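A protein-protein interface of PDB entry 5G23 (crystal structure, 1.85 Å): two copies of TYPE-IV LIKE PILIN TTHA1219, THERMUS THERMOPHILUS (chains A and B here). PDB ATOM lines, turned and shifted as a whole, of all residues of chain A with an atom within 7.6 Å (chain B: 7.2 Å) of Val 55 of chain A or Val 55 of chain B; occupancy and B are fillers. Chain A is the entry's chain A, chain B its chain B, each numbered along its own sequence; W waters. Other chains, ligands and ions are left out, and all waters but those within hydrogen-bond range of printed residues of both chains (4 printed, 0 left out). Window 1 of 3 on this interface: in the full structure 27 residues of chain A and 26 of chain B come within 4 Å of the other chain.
The guanidinium group (NH2) of Arg 58 of chain B lies within hydrogen-bond range of the backbone carbonyl oxygen (O) of Arg 58 of chain A.
NH1 of Arg 58 of chain A lies within salt-bridge range of OE1 of Glu 59 of chain B, at 3.2 Å.
OE1 of Glu 59 of chain A is in salt-bridge range of NH1 of Arg 58 of chain B (2.9 Å).
The side-chain hydroxyl (OG1) of Thr 54 of chain A sits at hydrogen-bond distance from the backbone carbonyl oxygen (O) of Ser 50 of chain A.
Among the printed residues, merely in contact across the chains: Arg 58 of chain A with Trp 118 of chain B (3.4 Å), Leu 51 of chain A with Thr 52 of chain B (3.5 Å), Thr 52 of chain A with Leu 51 of chain B (3.5 Å), Val 134 of chain A with Leu 51 of chain B (3.7 Å), Val 55 of chain A with Val 55 of chain B (3.7 Å), Leu 51 of chain A with Val 134 of chain B (3.7 Å), Thr 54 of chain A with Val 55 of chain B (3.8 Å) and Arg 58 of chain A with Val 55 of chain B (3.9 Å).
Val 55 of chain A touches one residue of chain B.
Of chain A, only Thr 54, Val 55 and Arg 58 come within 4 Å of Val 55 of chain B.
Printed residues of chain B within 4 Å of Val 134 of chain A: Leu 51 (3.7 Å).
Printed residues of chain A within 4 Å of Leu 51 of chain B: Thr 52 (3.5 Å) and Val 134 (3.7 Å).
Of the printed residues of chain A, Trp 118 of chain B touches Arg 58 (3.4 Å).
Of the printed residues of chain A, Glu 59 of chain B touches Arg 58.
Ala 53 of chain A touches none of the printed residues of chain B.
Hydrophobic or aromatic side chains of chain B that line the printed part of chain A: Leu 51, Val 55, Trp 118 and Val 134.
Along chain B the printed residues that touch a printed residue of chain A span positions 51 to 134.
Among the printed residues, 11 pairs touch across the chains.
Among the printed residues, Asp or Glu carboxylates within 4 Å of a Lys or Arg side-chain nitrogen of the other chain: Arg 58 of chain A with Glu 59 of chain B (3.2 Å) and Glu 59 of chain A with Arg 58 of chain B (2.9 Å).
Thr 54 of chain A touches Val 55 of chain B, but with the chains exchanged Val 55 of chain A does not touch Thr 54 of chain B (4.1 Å).
Arg 58 of chain A touches Val 55 of chain B, but with the chains exchanged Val 55 of chain A does not touch Arg 58 of chain B (5.1 Å).
Arg 58 of chain B touches its own counterpart, Arg 58 of chain A.
Arg 58 of chain A touches Trp 118 of chain B, but with the chains exchanged Trp 118 of chain A does not touch Arg 58 of chain B (7.3 Å).
Water W1 bridges NH1 of Arg 58 of chain A (2.6 Å) and O of Val 55 of chain B (2.8 Å).
Water W4 lies within hydrogen-bond range of the backbone carbonyl oxygen (O) of Val 55 of chain A (2.7 Å) and the guanidinium group (NH1) of Arg 58 of chain B (3.2 Å).
Water W2 lies within hydrogen-bond range of OH of Tyr 109 of chain B, NH1 of Arg 58 of chain A and NE1 of Trp 118 of chain B.
Water W3 bridges NH2 of Arg 58 of chain B (3.0 Å) and OE1 of Glu 59 of chain A (3.4 Å).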
ATOM      1  N   LEU A  49       3.563  -8.091 -24.933  1.00  0.00           N
ATOM      2  CA  LEU A  49       3.475  -7.480 -23.595  1.00  0.00           C
ATOM      3  C   LEU A  49       2.081  -6.894 -23.304  1.00  0.00           C
ATOM      4  O   LEU A  49       1.608  -7.057 -22.201  1.00  0.00           O
ATOM      5  CB  LEU A  49       4.505  -6.392 -23.407  1.00  0.00           C
ATOM      6  CG  LEU A  49       5.954  -6.880 -23.424  1.00  0.00           C
ATOM      7  CD1 LEU A  49       6.899  -5.707 -23.276  1.00  0.00           C
ATOM      8  CD2 LEU A  49       6.252  -7.884 -22.337  1.00  0.00           C
ATOM      9  N   SER A  50       1.437  -6.249 -24.294  1.00  0.00           N
ATOM     10  CA  SER A  50       0.065  -5.790 -24.129  1.00  0.00           C
ATOM     11  C   SER A  50      -0.902  -6.933 -23.827  1.00  0.00           C
ATOM     12  O   SER A  50      -1.794  -6.765 -23.005  1.00  0.00           O
ATOM     13  CB  SER A  50      -0.454  -4.956 -25.324  1.00  0.00           C
ATOM     14  OG  SER A  50       0.442  -3.800 -25.329  1.00  0.00           O
ATOM     15  N   LEU A  51      -0.819  -8.034 -24.589  1.00  0.00           N
ATOM     16  CA  LEU A  51      -1.702  -9.173 -24.385  1.00  0.00           C
ATOM     17  C   LEU A  51      -1.507  -9.710 -22.959  1.00  0.00           C
ATOM     18  O   LEU A  51      -2.466 -10.019 -22.256  1.00  0.00           O
ATOM     19  CB  LEU A  51      -1.400 -10.319 -25.381  1.00  0.00           C
ATOM     20  CG  LEU A  51      -1.907 -10.061 -26.813  1.00  0.00           C
ATOM     21  CD1 LEU A  51      -1.289 -11.090 -27.732  1.00  0.00           C
ATOM     22  CD2 LEU A  51      -3.413 -10.233 -26.810  1.00  0.00           C
ATOM     23  N   THR A  52      -0.267  -9.778 -22.538  1.00  0.00           N
ATOM     24  CA  THR A  52       0.092 -10.317 -21.187  1.00  0.00           C
ATOM     25  C   THR A  52      -0.465  -9.412 -20.152  1.00  0.00           C
ATOM     26  O   THR A  52      -1.073  -9.848 -19.179  1.00  0.00           O
ATOM     27  CB  THR A  52       1.646 -10.394 -21.068  1.00  0.00           C
ATOM     28  OG1 THR A  52       2.139 -11.265 -22.094  1.00  0.00           O
ATOM     29  CG2 THR A  52       2.050 -10.913 -19.736  1.00  0.00           C
ATOM     30  N   ALA A  53      -0.352  -8.111 -20.353  1.00  0.00           N
ATOM     31  CA  ALA A  53      -0.902  -7.186 -19.381  1.00  0.00           C
ATOM     32  C   ALA A  53      -2.409  -7.335 -19.258  1.00  0.00           C
ATOM     33  O   ALA A  53      -2.980  -7.180 -18.187  1.00  0.00           O
ATOM     34  CB  ALA A  53      -0.540  -5.753 -19.738  1.00  0.00           C
ATOM     35  N   THR A  54      -3.068  -7.559 -20.368  1.00  0.00           N
ATOM     36  CA  THR A  54      -4.518  -7.680 -20.352  1.00  0.00           C
ATOM     37  C   THR A  54      -4.897  -8.909 -19.570  1.00  0.00           C
ATOM     38  O   THR A  54      -5.849  -8.895 -18.811  1.00  0.00           O
ATOM     39  CB  THR A  54      -5.081  -7.733 -21.770  1.00  0.00           C
ATOM     40  OG1 THR A  54      -4.741  -6.505 -22.439  1.00  0.00           O
ATOM     41  CG2 THR A  54      -6.640  -7.920 -21.811  1.00  0.00           C
ATOM     42  N   VAL A  55      -4.175 -10.000 -19.780  1.00  0.00           N
ATOM     43  CA  VAL A  55      -4.518 -11.262 -19.087  1.00  0.00           C
ATOM     44  C   VAL A  55      -4.371 -11.036 -17.581  1.00  0.00           C
ATOM     45  O   VAL A  55      -5.216 -11.406 -16.805  1.00  0.00           O
ATOM     46  CB  VAL A  55      -3.632 -12.409 -19.594  1.00  0.00           C
ATOM     47  CG1 VAL A  55      -3.790 -13.652 -18.714  1.00  0.00           C
ATOM     48  CG2 VAL A  55      -4.005 -12.749 -21.020  1.00  0.00           C
ATOM     49  N   LEU A  56      -3.267 -10.435 -17.159  1.00  0.00           N
ATOM     50  CA  LEU A  56      -2.980 -10.274 -15.736  1.00  0.00           C
ATOM     51  C   LEU A  56      -3.923  -9.280 -15.076  1.00  0.00           C
ATOM     52  O   LEU A  56      -4.363  -9.461 -13.946  1.00  0.00           O
ATOM     53  CB  LEU A  56      -1.507  -9.799 -15.538  1.00  0.00           C
ATOM     54  CG  LEU A  56      -0.506 -10.895 -15.289  1.00  0.00           C
ATOM     55  CD1 LEU A  56      -0.439 -11.821 -16.472  1.00  0.00           C
ATOM     56  CD2 LEU A  56       0.885 -10.314 -14.955  1.00  0.00           C
ATOM     57  N   ALA A  57      -4.223  -8.213 -15.801  1.00  0.00           N
ATOM     58  CA  ALA A  57      -5.111  -7.195 -15.251  1.00  0.00           C
ATOM     59  C   ALA A  57      -6.488  -7.718 -14.994  1.00  0.00           C
ATOM     60  O   ALA A  57      -7.071  -7.450 -13.962  1.00  0.00           O
ATOM     61  CB  ALA A  57      -5.191  -5.983 -16.196  1.00  0.00           C
ATOM     62  N   ARG A  58      -7.029  -8.470 -15.967  1.00  0.00           N
ATOM     63  CA  ARG A  58      -8.379  -8.949 -15.845  1.00  0.00           C
ATOM     64  C   ARG A  58      -8.443  -9.922 -14.659  1.00  0.00           C
ATOM     65  O   ARG A  58      -9.396  -9.966 -13.927  1.00  0.00           O
ATOM     66  CB  ARG A  58      -8.918  -9.465 -17.197  1.00  0.00           C
ATOM     67  CG  ARG A  58      -9.169  -8.217 -18.040  1.00  0.00           C
ATOM     68  CD  ARG A  58      -9.746  -8.376 -19.397  1.00  0.00           C
ATOM     69  NE  ARG A  58      -9.827  -7.057 -20.058  1.00  0.00           N
ATOM     70  CZ  ARG A  58     -10.090  -6.901 -21.362  1.00  0.00           C
ATOM     71  NH1 ARG A  58     -10.372  -7.949 -22.169  1.00  0.00           N
ATOM     72  NH2 ARG A  58     -10.096  -5.661 -21.871  1.00  0.00           N
ATOM     73  N   GLU A  59      -7.421 -10.685 -14.442  1.00  0.00           N
ATOM     74  CA  GLU A  59      -7.403 -11.607 -13.334  1.00  0.00           C
ATOM     75  C   GLU A  59      -7.191 -10.922 -11.972  1.00  0.00           C
ATOM     76  O   GLU A  59      -7.816 -11.280 -10.984  1.00  0.00           O
ATOM     77  CB  GLU A  59      -6.270 -12.616 -13.597  1.00  0.00           C
ATOM     78  CG  GLU A  59      -6.048 -13.663 -12.565  1.00  0.00           C
ATOM     79  CD  GLU A  59      -6.924 -14.856 -12.780  1.00  0.00           C
ATOM     80  OE1 GLU A  59      -7.579 -14.940 -13.861  1.00  0.00           O
ATOM     81  OE2 GLU A  59      -6.933 -15.725 -11.906  1.00  0.00           O
ATOM     82  N   LEU A  60      -6.298  -9.954 -11.903  1.00  0.00           N
ATOM     83  CA  LEU A  60      -5.993  -9.300 -10.632  1.00  0.00           C
ATOM     84  C   LEU A  60      -7.084  -8.357 -10.176  1.00  0.00           C
ATOM     85  O   LEU A  60      -7.258  -8.112  -8.950  1.00  0.00           O
ATOM     86  CB  LEU A  60      -4.625  -8.584 -10.676  1.00  0.00           C
ATOM     87  CG  LEU A  60      -3.483  -9.601 -10.757  1.00  0.00           C
ATOM     88  CD1 LEU A  60      -2.187  -8.915 -11.031  1.00  0.00           C
ATOM     89  CD2 LEU A  60      -3.328 -10.437  -9.491  1.00  0.00           C
ATOM     90  N   TYR A  61      -7.842  -7.810 -11.119  1.00  0.00           N
ATOM     91  CA  TYR A  61      -8.961  -6.959 -10.784  1.00  0.00           C
ATOM     92  C   TYR A  61      -9.994  -7.680  -9.926  1.00  0.00           C
ATOM     93  O   TYR A  61     -10.610  -7.062  -9.096  1.00  0.00           O
ATOM     94  CB  TYR A  61      -9.690  -6.495 -12.092  1.00  0.00           C
ATOM     95  CG  TYR A  61     -10.795  -5.553 -11.858  1.00  0.00           C
ATOM     96  CD1 TYR A  61     -10.553  -4.174 -11.756  1.00  0.00           C
ATOM     97  CD2 TYR A  61     -12.096  -6.002 -11.739  1.00  0.00           C
ATOM     98  CE1 TYR A  61     -11.587  -3.261 -11.556  1.00  0.00           C
ATOM     99  CE2 TYR A  61     -13.153  -5.097 -11.543  1.00  0.00           C
ATOM    100  CZ  TYR A  61     -12.871  -3.744 -11.433  1.00  0.00           C
ATOM    101  OH  TYR A  61     -13.936  -2.842 -11.254  1.00  0.00           O
ATOM    102  N   TYR A 109       1.338 -15.180  -9.872  1.00  0.00           N
ATOM    103  CA  TYR A 109       2.280 -14.908 -10.913  1.00  0.00           C
ATOM    104  C   TYR A 109       3.703 -14.682 -10.381  1.00  0.00           C
ATOM    105  O   TYR A 109       3.912 -14.010  -9.371  1.00  0.00           O
ATOM    106  CB  TYR A 109       1.854 -13.658 -11.665  1.00  0.00           C
ATOM    107  CG  TYR A 109       0.544 -13.746 -12.416  1.00  0.00           C
ATOM    108  CD1 TYR A 109       0.469 -14.342 -13.648  1.00  0.00           C
ATOM    109  CD2 TYR A 109      -0.589 -13.204 -11.887  1.00  0.00           C
ATOM    110  CE1 TYR A 109      -0.751 -14.428 -14.335  1.00  0.00           C
ATOM    111  CE2 TYR A 109      -1.790 -13.271 -12.567  1.00  0.00           C
ATOM    112  CZ  TYR A 109      -1.852 -13.900 -13.792  1.00  0.00           C
ATOM    113  OH  TYR A 109      -3.054 -13.900 -14.482  1.00  0.00           O
ATOM    114  N   TRP A 118       2.014 -18.503 -14.423  1.00  0.00           N
ATOM    115  CA  TRP A 118       0.802 -18.382 -13.713  1.00  0.00           C
ATOM    116  C   TRP A 118       0.455 -19.667 -12.997  1.00  0.00           C
ATOM    117  O   TRP A 118       0.656 -20.773 -13.530  1.00  0.00           O
ATOM    118  CB  TRP A 118      -0.305 -18.051 -14.712  1.00  0.00           C
ATOM    119  CG  TRP A 118      -1.619 -18.029 -14.170  1.00  0.00           C
ATOM    120  CD1 TRP A 118      -2.087 -17.189 -13.151  1.00  0.00           C
ATOM    121  CD2 TRP A 118      -2.730 -18.837 -14.558  1.00  0.00           C
ATOM    122  NE1 TRP A 118      -3.393 -17.461 -12.905  1.00  0.00           N
ATOM    123  CE2 TRP A 118      -3.821 -18.461 -13.741  1.00  0.00           C
ATOM    124  CE3 TRP A 118      -2.916 -19.850 -15.518  1.00  0.00           C
ATOM    125  CZ2 TRP A 118      -5.116 -19.069 -13.853  1.00  0.00           C
ATOM    126  CZ3 TRP A 118      -4.181 -20.466 -15.623  1.00  0.00           C
ATOM    127  CH2 TRP A 118      -5.269 -20.072 -14.791  1.00  0.00           C
ATOM    128  N   VAL A 134       3.132 -18.065 -19.249  1.00  0.00           N
ATOM    129  CA  VAL A 134       2.222 -17.046 -19.832  1.00  0.00           C
ATOM    130  C   VAL A 134       2.967 -16.438 -21.008  1.00  0.00           C
ATOM    131  O   VAL A 134       2.429 -16.315 -22.122  1.00  0.00           O
ATOM    132  CB  VAL A 134       1.994 -15.943 -18.739  1.00  0.00           C
ATOM    133  CG1 VAL A 134       1.280 -14.738 -19.281  1.00  0.00           C
ATOM    134  CG2 VAL A 134       1.212 -16.528 -17.605  1.00  0.00           C
ATOM    135  N   TRP A 227       1.710  -0.945 -16.384  1.00  0.00           N
ATOM    136  CA  TRP A 227       0.249  -0.780 -16.437  1.00  0.00           C
ATOM    137  C   TRP A 227      -0.314  -0.785 -15.039  1.00  0.00           C
ATOM    138  O   TRP A 227       0.260  -1.382 -14.131  1.00  0.00           O
ATOM    139  CB  TRP A 227      -0.441  -1.772 -17.366  1.00  0.00           C
ATOM    140  CG  TRP A 227      -0.471  -3.230 -16.927  1.00  0.00           C
ATOM    141  CD1 TRP A 227      -1.573  -3.889 -16.559  1.00  0.00           C
ATOM    142  CD2 TRP A 227       0.596  -4.185 -16.899  1.00  0.00           C
ATOM    143  NE1 TRP A 227      -1.284  -5.153 -16.249  1.00  0.00           N
ATOM    144  CE2 TRP A 227       0.053  -5.388 -16.431  1.00  0.00           C
ATOM    145  CE3 TRP A 227       1.954  -4.140 -17.209  1.00  0.00           C
ATOM    146  CZ2 TRP A 227       0.797  -6.579 -16.307  1.00  0.00           C
ATOM    147  CZ3 TRP A 227       2.714  -5.327 -17.101  1.00  0.00           C
ATOM    148  CH2 TRP A 227       2.121  -6.542 -16.654  1.00  0.00           C
ATOM    149  N   LEU B  49      -0.762 -16.716 -29.611  1.00  0.00           N
ATOM    150  CA  LEU B  49      -2.126 -17.118 -29.945  1.00  0.00           C
ATOM    151  C   LEU B  49      -2.851 -17.592 -28.660  1.00  0.00           C
ATOM    152  O   LEU B  49      -4.081 -17.309 -28.520  1.00  0.00           O
ATOM    153  CB  LEU B  49      -2.176 -18.215 -30.982  1.00  0.00           C
ATOM    154  CG  LEU B  49      -1.690 -17.840 -32.377  1.00  0.00           C
ATOM    155  CD1 LEU B  49      -1.737 -19.012 -33.307  1.00  0.00           C
ATOM    156  CD2 LEU B  49      -2.509 -16.692 -32.997  1.00  0.00           C
ATOM    157  N   SER B  50      -2.166 -18.290 -27.780  1.00  0.00           N
ATOM    158  CA  SER B  50      -2.799 -18.721 -26.492  1.00  0.00           C
ATOM    159  C   SER B  50      -3.186 -17.508 -25.608  1.00  0.00           C
ATOM    160  O   SER B  50      -4.259 -17.506 -25.084  1.00  0.00           O
ATOM    161  CB  SER B  50      -1.911 -19.673 -25.700  1.00  0.00           C
ATOM    162  OG  SER B  50      -1.806 -20.860 -26.523  1.00  0.00           O
ATOM    163  N   LEU B  51      -2.339 -16.481 -25.555  1.00  0.00           N
ATOM    164  CA  LEU B  51      -2.661 -15.267 -24.845  1.00  0.00           C
ATOM    165  C   LEU B  51      -3.923 -14.647 -25.465  1.00  0.00           C
ATOM    166  O   LEU B  51      -4.805 -14.169 -24.742  1.00  0.00           O
ATOM    167  CB  LEU B  51      -1.487 -14.295 -24.884  1.00  0.00           C
ATOM    168  CG  LEU B  51      -0.301 -14.621 -23.979  1.00  0.00           C
ATOM    169  CD1 LEU B  51       0.857 -13.706 -24.324  1.00  0.00           C
ATOM    170  CD2 LEU B  51      -0.666 -14.418 -22.537  1.00  0.00           C
ATOM    171  N   THR B  52      -3.959 -14.596 -26.795  1.00  0.00           N
ATOM    172  CA  THR B  52      -5.040 -13.946 -27.522  1.00  0.00           C
ATOM    173  C   THR B  52      -6.324 -14.675 -27.242  1.00  0.00           C
ATOM    174  O   THR B  52      -7.371 -14.078 -26.941  1.00  0.00           O
ATOM    175  CB  THR B  52      -4.732 -13.932 -29.068  1.00  0.00           C
ATOM    176  OG1 THR B  52      -3.546 -13.199 -29.295  1.00  0.00           O
ATOM    177  CG2 THR B  52      -5.817 -13.274 -29.845  1.00  0.00           C
ATOM    178  N   ALA B  53      -6.262 -16.000 -27.251  1.00  0.00           N
ATOM    179  CA  ALA B  53      -7.462 -16.753 -26.945  1.00  0.00           C
ATOM    180  C   ALA B  53      -7.969 -16.559 -25.513  1.00  0.00           C
ATOM    181  O   ALA B  53      -9.189 -16.495 -25.306  1.00  0.00           O
ATOM    182  CB  ALA B  53      -7.211 -18.233 -27.172  1.00  0.00           C
ATOM    183  N   THR B  54      -7.061 -16.439 -24.559  1.00  0.00           N
ATOM    184  CA  THR B  54      -7.454 -16.195 -23.147  1.00  0.00           C
ATOM    185  C   THR B  54      -8.139 -14.847 -23.048  1.00  0.00           C
ATOM    186  O   THR B  54      -9.169 -14.759 -22.402  1.00  0.00           O
ATOM    187  CB  THR B  54      -6.234 -16.222 -22.241  1.00  0.00           C
ATOM    188  OG1 THR B  54      -5.617 -17.519 -22.363  1.00  0.00           O
ATOM    189  CG2 THR B  54      -6.552 -15.900 -20.786  1.00  0.00           C
ATOM    190  N   VAL B  55      -7.640 -13.822 -23.794  1.00  0.00           N
ATOM    191  CA  VAL B  55      -8.277 -12.499 -23.716  1.00  0.00           C
ATOM    192  C   VAL B  55      -9.682 -12.575 -24.267  1.00  0.00           C
ATOM    193  O   VAL B  55     -10.609 -12.072 -23.689  1.00  0.00           O
ATOM    194  CB  VAL B  55      -7.428 -11.439 -24.443  1.00  0.00           C
ATOM    195  CG1 VAL B  55      -8.144 -10.093 -24.580  1.00  0.00           C
ATOM    196  CG2 VAL B  55      -6.086 -11.212 -23.690  1.00  0.00           C
ATOM    197  N   LEU B  56      -9.844 -13.142 -25.466  1.00  0.00           N
ATOM    198  CA  LEU B  56     -11.138 -13.164 -26.121  1.00  0.00           C
ATOM    199  C   LEU B  56     -12.128 -14.044 -25.412  1.00  0.00           C
ATOM    200  O   LEU B  56     -13.331 -13.690 -25.328  1.00  0.00           O
ATOM    201  CB  LEU B  56     -10.976 -13.578 -27.595  1.00  0.00           C
ATOM    202  CG  LEU B  56     -10.757 -12.485 -28.636  1.00  0.00           C
ATOM    203  CD1 LEU B  56      -9.431 -11.750 -28.373  1.00  0.00           C
ATOM    204  CD2 LEU B  56     -10.749 -13.098 -30.059  1.00  0.00           C
ATOM    205  N   ALA B  57     -11.680 -15.187 -24.885  1.00  0.00           N
ATOM    206  CA  ALA B  57     -12.588 -16.078 -24.211  1.00  0.00           C
ATOM    207  C   ALA B  57     -13.160 -15.495 -22.981  1.00  0.00           C
ATOM    208  O   ALA B  57     -14.371 -15.602 -22.718  1.00  0.00           O
ATOM    209  CB  ALA B  57     -11.931 -17.372 -23.860  1.00  0.00           C
ATOM    210  N   ARG B  58     -12.319 -14.791 -22.227  1.00  0.00           N
ATOM    211  CA  ARG B  58     -12.802 -14.206 -20.978  1.00  0.00           C
ATOM    212  C   ARG B  58     -13.840 -13.145 -21.252  1.00  0.00           C
ATOM    213  O   ARG B  58     -14.812 -13.004 -20.520  1.00  0.00           O
ATOM    214  CB  ARG B  58     -11.651 -13.638 -20.169  1.00  0.00           C
ATOM    215  CG  ARG B  58     -12.029 -13.232 -18.759  1.00  0.00           C
ATOM    216  CD  ARG B  58     -10.905 -12.569 -17.914  1.00  0.00           C
ATOM    217  NE  ARG B  58     -11.367 -12.401 -16.508  1.00  0.00           N
ATOM    218  CZ  ARG B  58     -10.786 -12.884 -15.412  1.00  0.00           C
ATOM    219  NH1 ARG B  58      -9.607 -13.549 -15.477  1.00  0.00           N
ATOM    220  NH2 ARG B  58     -11.351 -12.666 -14.227  1.00  0.00           N
ATOM    221  N   GLU B  59     -13.636 -12.377 -22.305  1.00  0.00           N
ATOM    222  CA  GLU B  59     -14.532 -11.334 -22.638  1.00  0.00           C
ATOM    223  C   GLU B  59     -15.870 -11.893 -23.196  1.00  0.00           C
ATOM    224  O   GLU B  59     -16.939 -11.383 -22.887  1.00  0.00           O
ATOM    225  CB  GLU B  59     -13.801 -10.440 -23.636  1.00  0.00           C
ATOM    226  CG  GLU B  59     -14.516  -9.227 -24.149  1.00  0.00           C
ATOM    227  CD  GLU B  59     -14.361  -8.055 -23.238  1.00  0.00           C
ATOM    228  OE1 GLU B  59     -13.593  -8.164 -22.256  1.00  0.00           O
ATOM    229  OE2 GLU B  59     -15.121  -7.103 -23.453  1.00  0.00           O
ATOM    230  N   LEU B  60     -15.808 -12.880 -24.068  1.00  0.00           N
ATOM    231  CA  LEU B  60     -16.985 -13.368 -24.746  1.00  0.00           C
ATOM    232  C   LEU B  60     -17.863 -14.265 -23.847  1.00  0.00           C
ATOM    233  O   LEU B  60     -19.078 -14.317 -24.062  1.00  0.00           O
ATOM    234  CB  LEU B  60     -16.619 -14.083 -26.049  1.00  0.00           C
ATOM    235  CG  LEU B  60     -16.040 -13.119 -27.105  1.00  0.00           C
ATOM    236  CD1 LEU B  60     -15.465 -13.869 -28.286  1.00  0.00           C
ATOM    237  CD2 LEU B  60     -17.084 -12.112 -27.616  1.00  0.00           C
ATOM    238  N   TYR B 109     -14.734  -7.469 -31.822  1.00  0.00           N
ATOM    239  CA  TYR B 109     -13.510  -7.895 -32.401  1.00  0.00           C
ATOM    240  C   TYR B 109     -13.680  -7.973 -33.904  1.00  0.00           C
ATOM    241  O   TYR B 109     -14.725  -8.435 -34.383  1.00  0.00           O
ATOM    242  CB  TYR B 109     -13.131  -9.293 -31.874  1.00  0.00           C
ATOM    243  CG  TYR B 109     -12.802  -9.283 -30.446  1.00  0.00           C
ATOM    244  CD1 TYR B 109     -11.514  -8.894 -30.026  1.00  0.00           C
ATOM    245  CD2 TYR B 109     -13.680  -9.722 -29.515  1.00  0.00           C
ATOM    246  CE1 TYR B 109     -11.199  -8.874 -28.686  1.00  0.00           C
ATOM    247  CE2 TYR B 109     -13.370  -9.715 -28.171  1.00  0.00           C
ATOM    248  CZ  TYR B 109     -12.132  -9.282 -27.769  1.00  0.00           C
ATOM    249  OH  TYR B 109     -11.796  -9.344 -26.436  1.00  0.00           O
ATOM    250  N   TRP B 118      -9.768  -4.791 -31.381  1.00  0.00           N
ATOM    251  CA  TRP B 118     -10.791  -4.810 -30.392  1.00  0.00           C
ATOM    252  C   TRP B 118     -11.342  -3.443 -30.114  1.00  0.00           C
ATOM    253  O   TRP B 118     -10.580  -2.419 -30.138  1.00  0.00           O
ATOM    254  CB  TRP B 118     -10.188  -5.346 -29.075  1.00  0.00           C
ATOM    255  CG  TRP B 118     -11.122  -5.285 -27.887  1.00  0.00           C
ATOM    256  CD1 TRP B 118     -12.346  -5.923 -27.721  1.00  0.00           C
ATOM    257  CD2 TRP B 118     -10.922  -4.527 -26.690  1.00  0.00           C
ATOM    258  NE1 TRP B 118     -12.873  -5.649 -26.485  1.00  0.00           N
ATOM    259  CE2 TRP B 118     -12.031  -4.788 -25.835  1.00  0.00           C
ATOM    260  CE3 TRP B 118      -9.878  -3.710 -26.230  1.00  0.00           C
ATOM    261  CZ2 TRP B 118     -12.172  -4.187 -24.588  1.00  0.00           C
ATOM    262  CZ3 TRP B 118     -10.011  -3.112 -24.922  1.00  0.00           C
ATOM    263  CH2 TRP B 118     -11.154  -3.362 -24.147  1.00  0.00           C
ATOM    264  N   VAL B 134      -4.927  -5.945 -31.071  1.00  0.00           N
ATOM    265  CA  VAL B 134      -4.766  -7.111 -30.228  1.00  0.00           C
ATOM    266  C   VAL B 134      -3.516  -7.866 -30.667  1.00  0.00           C
ATOM    267  O   VAL B 134      -2.601  -8.069 -29.889  1.00  0.00           O
ATOM    268  CB  VAL B 134      -6.021  -8.046 -30.333  1.00  0.00           C
ATOM    269  CG1 VAL B 134      -5.865  -9.315 -29.472  1.00  0.00           C
ATOM    270  CG2 VAL B 134      -7.245  -7.284 -29.834  1.00  0.00           C
ATOM    271  N   TRP B 227     -10.440 -22.547 -30.352  1.00  0.00           N
ATOM    272  CA  TRP B 227     -10.891 -22.658 -28.992  1.00  0.00           C
ATOM    273  C   TRP B 227     -12.411 -22.458 -28.901  1.00  0.00           C
ATOM    274  O   TRP B 227     -12.972 -21.752 -29.734  1.00  0.00           O
ATOM    275  CB  TRP B 227     -10.065 -21.762 -28.071  1.00  0.00           C
ATOM    276  CG  TRP B 227     -10.261 -20.275 -28.185  1.00  0.00           C
ATOM    277  CD1 TRP B 227     -10.829 -19.537 -27.266  1.00  0.00           C
ATOM    278  CD2 TRP B 227      -9.787 -19.385 -29.181  1.00  0.00           C
ATOM    279  NE1 TRP B 227     -10.833 -18.234 -27.614  1.00  0.00           N
ATOM    280  CE2 TRP B 227     -10.182 -18.110 -28.806  1.00  0.00           C
ATOM    281  CE3 TRP B 227      -9.129 -19.546 -30.412  1.00  0.00           C
ATOM    282  CZ2 TRP B 227      -9.919 -16.986 -29.574  1.00  0.00           C
ATOM    283  CZ3 TRP B 227      -8.785 -18.425 -31.154  1.00  0.00           C
ATOM    284  CH2 TRP B 227      -9.203 -17.142 -30.750  1.00  0.00           C
HETATM  285  O   HOH W   1     -10.227 -10.483 -21.450  1.00  0.00           O
HETATM  286  O   HOH W   2     -10.183  -7.363 -25.419  1.00  0.00           O
HETATM  287  O   HOH W   3     -10.270 -14.158 -11.880  1.00  0.00           O
HETATM  288  O   HOH W   4      -7.317 -12.936 -17.695  1.00  0.00           O
